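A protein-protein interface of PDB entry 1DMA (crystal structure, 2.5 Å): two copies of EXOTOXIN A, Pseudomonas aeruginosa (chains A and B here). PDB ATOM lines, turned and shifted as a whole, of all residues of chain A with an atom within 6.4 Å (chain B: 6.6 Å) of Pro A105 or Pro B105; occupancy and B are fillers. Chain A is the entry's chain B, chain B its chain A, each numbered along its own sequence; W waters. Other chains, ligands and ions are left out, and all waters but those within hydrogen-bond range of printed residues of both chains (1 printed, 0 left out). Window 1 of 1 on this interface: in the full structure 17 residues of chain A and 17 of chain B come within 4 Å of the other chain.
Pro A105 touches just these residues of chain B: Pro B105 (3.8 Å) and Ser B107 (3.2 Å). Pro B105 touches two residues of chain A. Printed residues of chain A within 4 Å of Arg B164: Tyr A35, Arg A164 and Thr A165. Printed residues of chain B within 4 Å of Ser A107: Gly B34, Pro B105, Arg B106 and Ser B107. Of the printed residues of chain A, Arg B106 touches Ser A107 (3.7 Å). Of the printed residues of chain A, Thr B165 touches Arg A164. Ser B108 touches none of the printed residues of chain A. The nearest printed residue of chain B that does not touch Pro A105 is Tyr B35 (5.0 Å). The nearest printed residue of chain B that does not touch Ser A107 is Ser B108 (5.1 Å).
The backbone carbonyl oxygen (O) of Gly B34 lies within hydrogen-bond range of the backbone NH (N) of Arg B106 (2.9 Å). The backbone carbonyl oxygen (O) of Gly A34 sits at hydrogen-bond distance from the backbone NH (N) of Arg A106. The backbone carbonyl oxygen (O) of Pro A105 lies within hydrogen-bond range of the side-chain hydroxyl (OG) of Ser A108, at 2.7 Å.
Pro A105 touches its own counterpart, Pro B105. Pro A105 touches Ser B107, and with the chains exchanged Ser A107 touches Pro B105. Ser A107 touches its own counterpart, Ser B107. Arg A164 touches Thr B165, and with the chains exchanged Thr A165 touches Arg B164. Of the 14 pairs that touch across the chains among the printed residues, 13 have their exchanged pair printed and touching as well.
Among the printed residues, merely in contact across the chains: Arg A33 with Ser B107 (3.7 Å), Gly A34 with Ser B107 (3.6 Å), Tyr A35 with Arg B164 (3.5 Å), Pro A105 with Pro B105 (3.8 Å), Pro A105 with Ser B107 (3.2 Å), Ser A107 with Gly B34 (3.7 Å), Ser A107 with Pro B105 (3.9 Å), Ser A107 with Arg B106 (3.7 Å), Arg A164 with Tyr B35 (3.8 Å) and Arg A164 with Arg B164 (3.7 Å).
OG of Ser B107 lies within hydrogen-bond range of N of Arg A106 (3.4 Å). OG of Ser A107 is in hydrogen-bond range of OG of Ser B107 (2.8 Å). The backbone carbonyl oxygen (O) of Thr A165 is in hydrogen-bond range of the guanidinium group (NH1) of Arg B164 (2.8 Å). O of Thr B165 lies within hydrogen-bond range of NE of Arg A164, at 2.9 Å.
Of the 15 printed residues of chain A, 8 touch a printed residue of chain B. Printed residues of chain A that touch a printed residue of chain B: Arg A33, Gly A34, Tyr A35, Pro A105, Arg A106, Ser A107, Arg A164 and Thr A165. Hydrophobic or aromatic side chains of chain A within 4 Å of the printed part of chain B: Tyr A35 and Pro A105. Of the 15 printed residues of chain B, 7 touch a printed residue of chain A. Among the printed residues, no Asp or Glu carboxylate lies within 4 Å of a Lys or Arg side-chain nitrogen of the other chain.
Water W1 lies within hydrogen-bond range of the backbone carbonyl oxygen (O) of Arg A33 and the side-chain hydroxyl (OG) of Ser B108.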
ATOM      1  N   ARG A  33      -3.554  17.030  35.964  1.00  0.00           N
ATOM      2  CA  ARG A  33      -2.158  16.824  35.818  1.00  0.00           C
ATOM      3  C   ARG A  33      -1.623  17.509  34.597  1.00  0.00           C
ATOM      4  O   ARG A  33      -0.558  17.182  34.120  1.00  0.00           O
ATOM      5  CB  ARG A  33      -1.872  15.358  35.783  1.00  0.00           C
ATOM      6  CG  ARG A  33      -1.858  14.824  37.177  1.00  0.00           C
ATOM      7  CD  ARG A  33      -0.864  15.622  38.052  1.00  0.00           C
ATOM      8  NE  ARG A  33      -0.810  15.052  39.397  1.00  0.00           N
ATOM      9  CZ  ARG A  33      -1.547  15.466  40.428  1.00  0.00           C
ATOM     10  NH1 ARG A  33      -2.343  16.535  40.312  1.00  0.00           N
ATOM     11  NH2 ARG A  33      -1.441  14.842  41.597  1.00  0.00           N
ATOM     12  N   GLY A  34      -2.396  18.427  34.053  1.00  0.00           N
ATOM     13  CA  GLY A  34      -1.935  19.198  32.909  1.00  0.00           C
ATOM     14  C   GLY A  34      -2.123  18.721  31.483  1.00  0.00           C
ATOM     15  O   GLY A  34      -1.694  19.418  30.545  1.00  0.00           O
ATOM     16  N   TYR A  35      -2.755  17.563  31.308  1.00  0.00           N
ATOM     17  CA  TYR A  35      -3.005  17.007  29.982  1.00  0.00           C
ATOM     18  C   TYR A  35      -4.251  17.557  29.258  1.00  0.00           C
ATOM     19  O   TYR A  35      -5.250  17.900  29.876  1.00  0.00           O
ATOM     20  CB  TYR A  35      -3.060  15.472  30.096  1.00  0.00           C
ATOM     21  CG  TYR A  35      -1.678  14.850  30.155  1.00  0.00           C
ATOM     22  CD1 TYR A  35      -0.966  14.735  31.360  1.00  0.00           C
ATOM     23  CD2 TYR A  35      -1.028  14.507  28.979  1.00  0.00           C
ATOM     24  CE1 TYR A  35       0.371  14.311  31.370  1.00  0.00           C
ATOM     25  CE2 TYR A  35       0.292  14.082  28.973  1.00  0.00           C
ATOM     26  CZ  TYR A  35       1.000  13.988  30.154  1.00  0.00           C
ATOM     27  OH  TYR A  35       2.345  13.614  30.041  1.00  0.00           O
ATOM     28  N   VAL A  36      -4.178  17.702  27.948  1.00  0.00           N
ATOM     29  CA  VAL A  36      -5.320  18.169  27.180  1.00  0.00           C
ATOM     30  C   VAL A  36      -5.564  17.248  25.954  1.00  0.00           C
ATOM     31  O   VAL A  36      -4.611  16.822  25.284  1.00  0.00           O
ATOM     32  CB  VAL A  36      -5.122  19.607  26.751  1.00  0.00           C
ATOM     33  CG1 VAL A  36      -5.075  20.470  27.927  1.00  0.00           C
ATOM     34  CG2 VAL A  36      -3.820  19.777  26.102  1.00  0.00           C
ATOM     35  N   TYR A 103      -4.048  12.438  24.570  1.00  0.00           N
ATOM     36  CA  TYR A 103      -3.699  13.563  25.471  1.00  0.00           C
ATOM     37  C   TYR A 103      -2.252  14.009  25.445  1.00  0.00           C
ATOM     38  O   TYR A 103      -1.365  13.180  25.518  1.00  0.00           O
ATOM     39  CB  TYR A 103      -3.960  13.145  26.911  1.00  0.00           C
ATOM     40  CG  TYR A 103      -5.407  13.054  27.223  1.00  0.00           C
ATOM     41  CD1 TYR A 103      -6.114  11.909  26.917  1.00  0.00           C
ATOM     42  CD2 TYR A 103      -6.098  14.163  27.692  1.00  0.00           C
ATOM     43  CE1 TYR A 103      -7.471  11.865  27.037  1.00  0.00           C
ATOM     44  CE2 TYR A 103      -7.446  14.140  27.830  1.00  0.00           C
ATOM     45  CZ  TYR A 103      -8.137  12.990  27.489  1.00  0.00           C
ATOM     46  OH  TYR A 103      -9.509  12.978  27.530  1.00  0.00           O
ATOM     47  N   VAL A 104      -2.007  15.307  25.510  1.00  0.00           N
ATOM     48  CA  VAL A 104      -0.640  15.826  25.518  1.00  0.00           C
ATOM     49  C   VAL A 104      -0.540  16.872  26.626  1.00  0.00           C
ATOM     50  O   VAL A 104      -1.543  17.398  27.056  1.00  0.00           O
ATOM     51  CB  VAL A 104      -0.281  16.558  24.195  1.00  0.00           C
ATOM     52  CG1 VAL A 104      -0.173  15.550  22.957  1.00  0.00           C
ATOM     53  CG2 VAL A 104      -1.257  17.717  23.957  1.00  0.00           C
ATOM     54  N   PRO A 105       0.659  17.123  27.173  1.00  0.00           N
ATOM     55  CA  PRO A 105       0.677  18.138  28.215  1.00  0.00           C
ATOM     56  C   PRO A 105       0.277  19.457  27.608  1.00  0.00           C
ATOM     57  O   PRO A 105       0.637  19.753  26.528  1.00  0.00           O
ATOM     58  CB  PRO A 105       2.128  18.122  28.660  1.00  0.00           C
ATOM     59  CG  PRO A 105       2.854  17.639  27.469  1.00  0.00           C
ATOM     60  CD  PRO A 105       1.996  16.530  27.002  1.00  0.00           C
ATOM     61  N   ARG A 106      -0.486  20.249  28.314  1.00  0.00           N
ATOM     62  CA  ARG A 106      -0.935  21.508  27.801  1.00  0.00           C
ATOM     63  C   ARG A 106       0.186  22.470  27.403  1.00  0.00           C
ATOM     64  O   ARG A 106      -0.069  23.468  26.742  1.00  0.00           O
ATOM     65  CB  ARG A 106      -1.877  22.121  28.844  1.00  0.00           C
ATOM     66  CG  ARG A 106      -2.098  23.617  28.763  1.00  0.00           C
ATOM     67  CD  ARG A 106      -3.407  23.968  29.449  1.00  0.00           C
ATOM     68  NE  ARG A 106      -4.550  23.467  28.677  1.00  0.00           N
ATOM     69  CZ  ARG A 106      -5.826  23.836  28.840  1.00  0.00           C
ATOM     70  NH1 ARG A 106      -6.178  24.706  29.791  1.00  0.00           N
ATOM     71  NH2 ARG A 106      -6.769  23.311  28.055  1.00  0.00           N
ATOM     72  N   SER A 107       1.432  22.123  27.713  1.00  0.00           N
ATOM     73  CA  SER A 107       2.586  23.002  27.428  1.00  0.00           C
ATOM     74  C   SER A 107       3.158  22.851  26.053  1.00  0.00           C
ATOM     75  O   SER A 107       3.918  23.695  25.583  1.00  0.00           O
ATOM     76  CB  SER A 107       3.751  22.744  28.409  1.00  0.00           C
ATOM     77  OG  SER A 107       3.293  22.313  29.675  1.00  0.00           O
ATOM     78  N   SER A 108       2.904  21.713  25.455  1.00  0.00           N
ATOM     79  CA  SER A 108       3.439  21.443  24.150  1.00  0.00           C
ATOM     80  C   SER A 108       2.590  22.028  23.066  1.00  0.00           C
ATOM     81  O   SER A 108       3.074  22.162  21.938  1.00  0.00           O
ATOM     82  CB  SER A 108       3.601  19.962  23.983  1.00  0.00           C
ATOM     83  OG  SER A 108       2.559  19.316  24.689  1.00  0.00           O
ATOM     84  N   LEU A 109       1.385  22.473  23.433  1.00  0.00           N
ATOM     85  CA  LEU A 109       0.479  23.096  22.483  1.00  0.00           C
ATOM     86  C   LEU A 109       1.142  24.240  21.642  1.00  0.00           C
ATOM     87  O   LEU A 109       0.702  24.530  20.535  1.00  0.00           O
ATOM     88  CB  LEU A 109      -0.822  23.536  23.153  1.00  0.00           C
ATOM     89  CG  LEU A 109      -1.695  22.446  23.767  1.00  0.00           C
ATOM     90  CD1 LEU A 109      -2.983  23.031  24.313  1.00  0.00           C
ATOM     91  CD2 LEU A 109      -2.028  21.408  22.800  1.00  0.00           C
ATOM     92  N   PHE A 112       2.185  23.082  18.131  1.00  0.00           N
ATOM     93  CA  PHE A 112       1.159  22.519  17.218  1.00  0.00           C
ATOM     94  C   PHE A 112       0.907  23.580  16.180  1.00  0.00           C
ATOM     95  O   PHE A 112       0.476  24.681  16.505  1.00  0.00           O
ATOM     96  CB  PHE A 112      -0.194  22.246  17.900  1.00  0.00           C
ATOM     97  CG  PHE A 112      -0.254  20.946  18.649  1.00  0.00           C
ATOM     98  CD1 PHE A 112       0.790  20.549  19.484  1.00  0.00           C
ATOM     99  CD2 PHE A 112      -1.350  20.116  18.527  1.00  0.00           C
ATOM    100  CE1 PHE A 112       0.737  19.341  20.180  1.00  0.00           C
ATOM    101  CE2 PHE A 112      -1.430  18.879  19.228  1.00  0.00           C
ATOM    102  CZ  PHE A 112      -0.393  18.495  20.050  1.00  0.00           C
ATOM    103  N   LEU A 161       6.850  13.407  20.554  1.00  0.00           N
ATOM    104  CA  LEU A 161       5.637  13.936  21.212  1.00  0.00           C
ATOM    105  C   LEU A 161       4.638  12.786  21.363  1.00  0.00           C
ATOM    106  O   LEU A 161       3.994  12.595  22.402  1.00  0.00           O
ATOM    107  CB  LEU A 161       4.963  14.967  20.289  1.00  0.00           C
ATOM    108  CG  LEU A 161       4.180  16.143  20.876  1.00  0.00           C
ATOM    109  CD1 LEU A 161       3.540  16.967  19.764  1.00  0.00           C
ATOM    110  CD2 LEU A 161       3.172  15.629  21.891  1.00  0.00           C
ATOM    111  N   ARG A 164       4.942  10.484  24.264  1.00  0.00           N
ATOM    112  CA  ARG A 164       4.856  11.098  25.576  1.00  0.00           C
ATOM    113  C   ARG A 164       3.468  11.654  25.772  1.00  0.00           C
ATOM    114  O   ARG A 164       3.275  12.678  26.429  1.00  0.00           O
ATOM    115  CB  ARG A 164       5.881  12.215  25.684  1.00  0.00           C
ATOM    116  CG  ARG A 164       7.291  11.726  25.835  1.00  0.00           C
ATOM    117  CD  ARG A 164       8.278  12.884  25.854  1.00  0.00           C
ATOM    118  NE  ARG A 164       9.632  12.405  26.034  1.00  0.00           N
ATOM    119  CZ  ARG A 164      10.367  11.889  25.070  1.00  0.00           C
ATOM    120  NH1 ARG A 164       9.949  11.898  23.816  1.00  0.00           N
ATOM    121  NH2 ARG A 164      11.569  11.447  25.347  1.00  0.00           N
ATOM    122  N   THR A 165       2.501  10.982  25.173  1.00  0.00           N
ATOM    123  CA  THR A 165       1.113  11.371  25.265  1.00  0.00           C
ATOM    124  C   THR A 165       0.507  10.294  26.154  1.00  0.00           C
ATOM    125  O   THR A 165       1.094   9.238  26.276  1.00  0.00           O
ATOM    126  CB  THR A 165       0.490  11.254  23.859  1.00  0.00           C
ATOM    127  OG1 THR A 165       0.678   9.922  23.374  1.00  0.00           O
ATOM    128  CG2 THR A 165       1.152  12.212  22.858  1.00  0.00           C
ATOM    129  N   GLY B  34       8.080  24.130  26.029  1.00  0.00           N
ATOM    130  CA  GLY B  34       7.367  23.733  27.250  1.00  0.00           C
ATOM    131  C   GLY B  34       8.000  22.807  28.295  1.00  0.00           C
ATOM    132  O   GLY B  34       7.298  22.257  29.176  1.00  0.00           O
ATOM    133  N   TYR B  35       9.307  22.599  28.206  1.00  0.00           N
ATOM    134  CA  TYR B  35       9.986  21.753  29.152  1.00  0.00           C
ATOM    135  C   TYR B  35      10.697  22.566  30.196  1.00  0.00           C
ATOM    136  O   TYR B  35      11.132  23.674  29.936  1.00  0.00           O
ATOM    137  CB  TYR B  35      10.924  20.816  28.437  1.00  0.00           C
ATOM    138  CG  TYR B  35      10.166  19.599  27.952  1.00  0.00           C
ATOM    139  CD1 TYR B  35       9.427  19.619  26.747  1.00  0.00           C
ATOM    140  CD2 TYR B  35      10.078  18.455  28.751  1.00  0.00           C
ATOM    141  CE1 TYR B  35       8.606  18.539  26.384  1.00  0.00           C
ATOM    142  CE2 TYR B  35       9.288  17.399  28.395  1.00  0.00           C
ATOM    143  CZ  TYR B  35       8.548  17.445  27.227  1.00  0.00           C
ATOM    144  OH  TYR B  35       7.676  16.417  26.991  1.00  0.00           O
ATOM    145  N   VAL B  36      10.661  22.067  31.424  1.00  0.00           N
ATOM    146  CA  VAL B  36      11.331  22.707  32.528  1.00  0.00           C
ATOM    147  C   VAL B  36      12.235  21.641  33.224  1.00  0.00           C
ATOM    148  O   VAL B  36      11.897  20.438  33.261  1.00  0.00           O
ATOM    149  CB  VAL B  36      10.312  23.331  33.461  1.00  0.00           C
ATOM    150  CG1 VAL B  36       9.438  22.291  34.023  1.00  0.00           C
ATOM    151  CG2 VAL B  36      11.016  24.032  34.577  1.00  0.00           C
ATOM    152  N   TYR B 103      14.243  16.687  32.262  1.00  0.00           N
ATOM    153  CA  TYR B 103      13.221  17.701  31.962  1.00  0.00           C
ATOM    154  C   TYR B 103      11.789  17.159  31.921  1.00  0.00           C
ATOM    155  O   TYR B 103      11.573  16.038  31.496  1.00  0.00           O
ATOM    156  CB  TYR B 103      13.534  18.334  30.619  1.00  0.00           C
ATOM    157  CG  TYR B 103      14.803  19.173  30.607  1.00  0.00           C
ATOM    158  CD1 TYR B 103      16.053  18.598  30.469  1.00  0.00           C
ATOM    159  CD2 TYR B 103      14.732  20.564  30.719  1.00  0.00           C
ATOM    160  CE1 TYR B 103      17.199  19.393  30.434  1.00  0.00           C
ATOM    161  CE2 TYR B 103      15.874  21.360  30.717  1.00  0.00           C
ATOM    162  CZ  TYR B 103      17.092  20.771  30.572  1.00  0.00           C
ATOM    163  OH  TYR B 103      18.213  21.575  30.661  1.00  0.00           O
ATOM    164  N   VAL B 104      10.816  17.906  32.438  1.00  0.00           N
ATOM    165  CA  VAL B 104       9.405  17.476  32.391  1.00  0.00           C
ATOM    166  C   VAL B 104       8.600  18.705  31.910  1.00  0.00           C
ATOM    167  O   VAL B 104       9.141  19.820  31.852  1.00  0.00           O
ATOM    168  CB  VAL B 104       8.830  16.959  33.778  1.00  0.00           C
ATOM    169  CG1 VAL B 104       9.738  15.955  34.423  1.00  0.00           C
ATOM    170  CG2 VAL B 104       8.515  18.102  34.695  1.00  0.00           C
ATOM    171  N   PRO B 105       7.340  18.505  31.452  1.00  0.00           N
ATOM    172  CA  PRO B 105       6.578  19.673  31.003  1.00  0.00           C
ATOM    173  C   PRO B 105       6.225  20.548  32.147  1.00  0.00           C
ATOM    174  O   PRO B 105       5.783  20.115  33.187  1.00  0.00           O
ATOM    175  CB  PRO B 105       5.287  19.074  30.445  1.00  0.00           C
ATOM    176  CG  PRO B 105       5.657  17.718  30.078  1.00  0.00           C
ATOM    177  CD  PRO B 105       6.622  17.257  31.136  1.00  0.00           C
ATOM    178  N   ARG B 106       6.236  21.809  31.846  1.00  0.00           N
ATOM    179  CA  ARG B 106       5.871  22.810  32.787  1.00  0.00           C
ATOM    180  C   ARG B 106       4.475  22.504  33.322  1.00  0.00           C
ATOM    181  O   ARG B 106       4.236  22.567  34.516  1.00  0.00           O
ATOM    182  CB  ARG B 106       5.943  24.153  32.054  1.00  0.00           C
ATOM    183  CG  ARG B 106       5.510  25.354  32.847  1.00  0.00           C
ATOM    184  CD  ARG B 106       6.234  26.598  32.378  1.00  0.00           C
ATOM    185  NE  ARG B 106       7.491  26.775  33.099  1.00  0.00           N
ATOM    186  CZ  ARG B 106       8.695  26.687  32.539  1.00  0.00           C
ATOM    187  NH1 ARG B 106       8.813  26.429  31.236  1.00  0.00           N
ATOM    188  NH2 ARG B 106       9.782  26.864  33.284  1.00  0.00           N
ATOM    189  N   SER B 107       3.600  21.999  32.469  1.00  0.00           N
ATOM    190  CA  SER B 107       2.220  21.711  32.871  1.00  0.00           C
ATOM    191  C   SER B 107       2.042  20.618  33.917  1.00  0.00           C
ATOM    192  O   SER B 107       1.010  20.518  34.600  1.00  0.00           O
ATOM    193  CB  SER B 107       1.332  21.472  31.634  1.00  0.00           C
ATOM    194  OG  SER B 107       1.739  20.370  30.855  1.00  0.00           O
ATOM    195  N   SER B 108       3.110  19.874  34.114  1.00  0.00           N
ATOM    196  CA  SER B 108       3.092  18.791  35.055  1.00  0.00           C
ATOM    197  C   SER B 108       3.488  19.225  36.432  1.00  0.00           C
ATOM    198  O   SER B 108       3.293  18.470  37.382  1.00  0.00           O
ATOM    199  CB  SER B 108       4.042  17.698  34.580  1.00  0.00           C
ATOM    200  OG  SER B 108       3.576  17.128  33.357  1.00  0.00           O
ATOM    201  N   LEU B 109       4.022  20.437  36.554  1.00  0.00           N
ATOM    202  CA  LEU B 109       4.482  20.918  37.851  1.00  0.00           C
ATOM    203  C   LEU B 109       3.505  20.880  39.024  1.00  0.00           C
ATOM    204  O   LEU B 109       3.894  20.898  40.197  1.00  0.00           O
ATOM    205  CB  LEU B 109       5.156  22.255  37.704  1.00  0.00           C
ATOM    206  CG  LEU B 109       6.542  22.053  37.089  1.00  0.00           C
ATOM    207  CD1 LEU B 109       7.144  23.406  36.799  1.00  0.00           C
ATOM    208  CD2 LEU B 109       7.457  21.316  38.013  1.00  0.00           C
ATOM    209  N   PRO B 110       2.213  20.880  38.726  1.00  0.00           N
ATOM    210  CA  PRO B 110       1.245  20.820  39.809  1.00  0.00           C
ATOM    211  C   PRO B 110       1.227  19.499  40.526  1.00  0.00           C
ATOM    212  O   PRO B 110       0.564  19.380  41.523  1.00  0.00           O
ATOM    213  CB  PRO B 110      -0.062  21.042  39.078  1.00  0.00           C
ATOM    214  CG  PRO B 110       0.339  22.097  38.139  1.00  0.00           C
ATOM    215  CD  PRO B 110       1.603  21.543  37.558  1.00  0.00           C
ATOM    216  N   PHE B 112       3.981  17.994  41.598  1.00  0.00           N
ATOM    217  CA  PHE B 112       5.277  17.930  42.258  1.00  0.00           C
ATOM    218  C   PHE B 112       5.062  18.535  43.643  1.00  0.00           C
ATOM    219  O   PHE B 112       4.787  19.730  43.746  1.00  0.00           O
ATOM    220  CB  PHE B 112       6.294  18.792  41.481  1.00  0.00           C
ATOM    221  CG  PHE B 112       7.163  18.005  40.488  1.00  0.00           C
ATOM    222  CD1 PHE B 112       6.665  17.638  39.228  1.00  0.00           C
ATOM    223  CD2 PHE B 112       8.503  17.691  40.795  1.00  0.00           C
ATOM    224  CE1 PHE B 112       7.463  16.993  38.298  1.00  0.00           C
ATOM    225  CE2 PHE B 112       9.321  17.048  39.866  1.00  0.00           C
ATOM    226  CZ  PHE B 112       8.789  16.694  38.604  1.00  0.00           C
ATOM    227  N   LEU B 161       5.198   9.401  35.006  1.00  0.00           N
ATOM    228  CA  LEU B 161       5.734  10.713  34.728  1.00  0.00           C
ATOM    229  C   LEU B 161       7.148  10.563  34.148  1.00  0.00           C
ATOM    230  O   LEU B 161       7.508  11.191  33.131  1.00  0.00           O
ATOM    231  CB  LEU B 161       5.815  11.483  36.053  1.00  0.00           C
ATOM    232  CG  LEU B 161       5.647  13.007  36.234  1.00  0.00           C
ATOM    233  CD1 LEU B 161       6.238  13.408  37.580  1.00  0.00           C
ATOM    234  CD2 LEU B 161       6.326  13.761  35.170  1.00  0.00           C
ATOM    235  N   ARG B 164       7.914   9.786  30.647  1.00  0.00           N
ATOM    236  CA  ARG B 164       7.554  10.905  29.784  1.00  0.00           C
ATOM    237  C   ARG B 164       8.458  12.136  29.930  1.00  0.00           C
ATOM    238  O   ARG B 164       8.067  13.260  29.573  1.00  0.00           O
ATOM    239  CB  ARG B 164       6.093  11.279  29.985  1.00  0.00           C
ATOM    240  CG  ARG B 164       5.165  10.302  29.270  1.00  0.00           C
ATOM    241  CD  ARG B 164       3.693  10.418  29.656  1.00  0.00           C
ATOM    242  NE  ARG B 164       3.351   9.221  30.397  1.00  0.00           N
ATOM    243  CZ  ARG B 164       2.710   8.178  29.900  1.00  0.00           C
ATOM    244  NH1 ARG B 164       2.178   8.213  28.691  1.00  0.00           N
ATOM    245  NH2 ARG B 164       2.513   7.134  30.675  1.00  0.00           N
ATOM    246  N   THR B 165       9.691  11.911  30.392  1.00  0.00           N
ATOM    247  CA  THR B 165      10.652  12.991  30.530  1.00  0.00           C
ATOM    248  C   THR B 165      11.515  13.080  29.297  1.00  0.00           C
ATOM    249  O   THR B 165      11.336  12.322  28.369  1.00  0.00           O
ATOM    250  CB  THR B 165      11.603  12.800  31.727  1.00  0.00           C
ATOM    251  OG1 THR B 165      12.150  11.492  31.704  1.00  0.00           O
ATOM    252  CG2 THR B 165      10.891  12.990  33.062  1.00  0.00           C
HETATM  253  O   HOH W   1       1.465  15.499  34.427  1.00  0.00           O
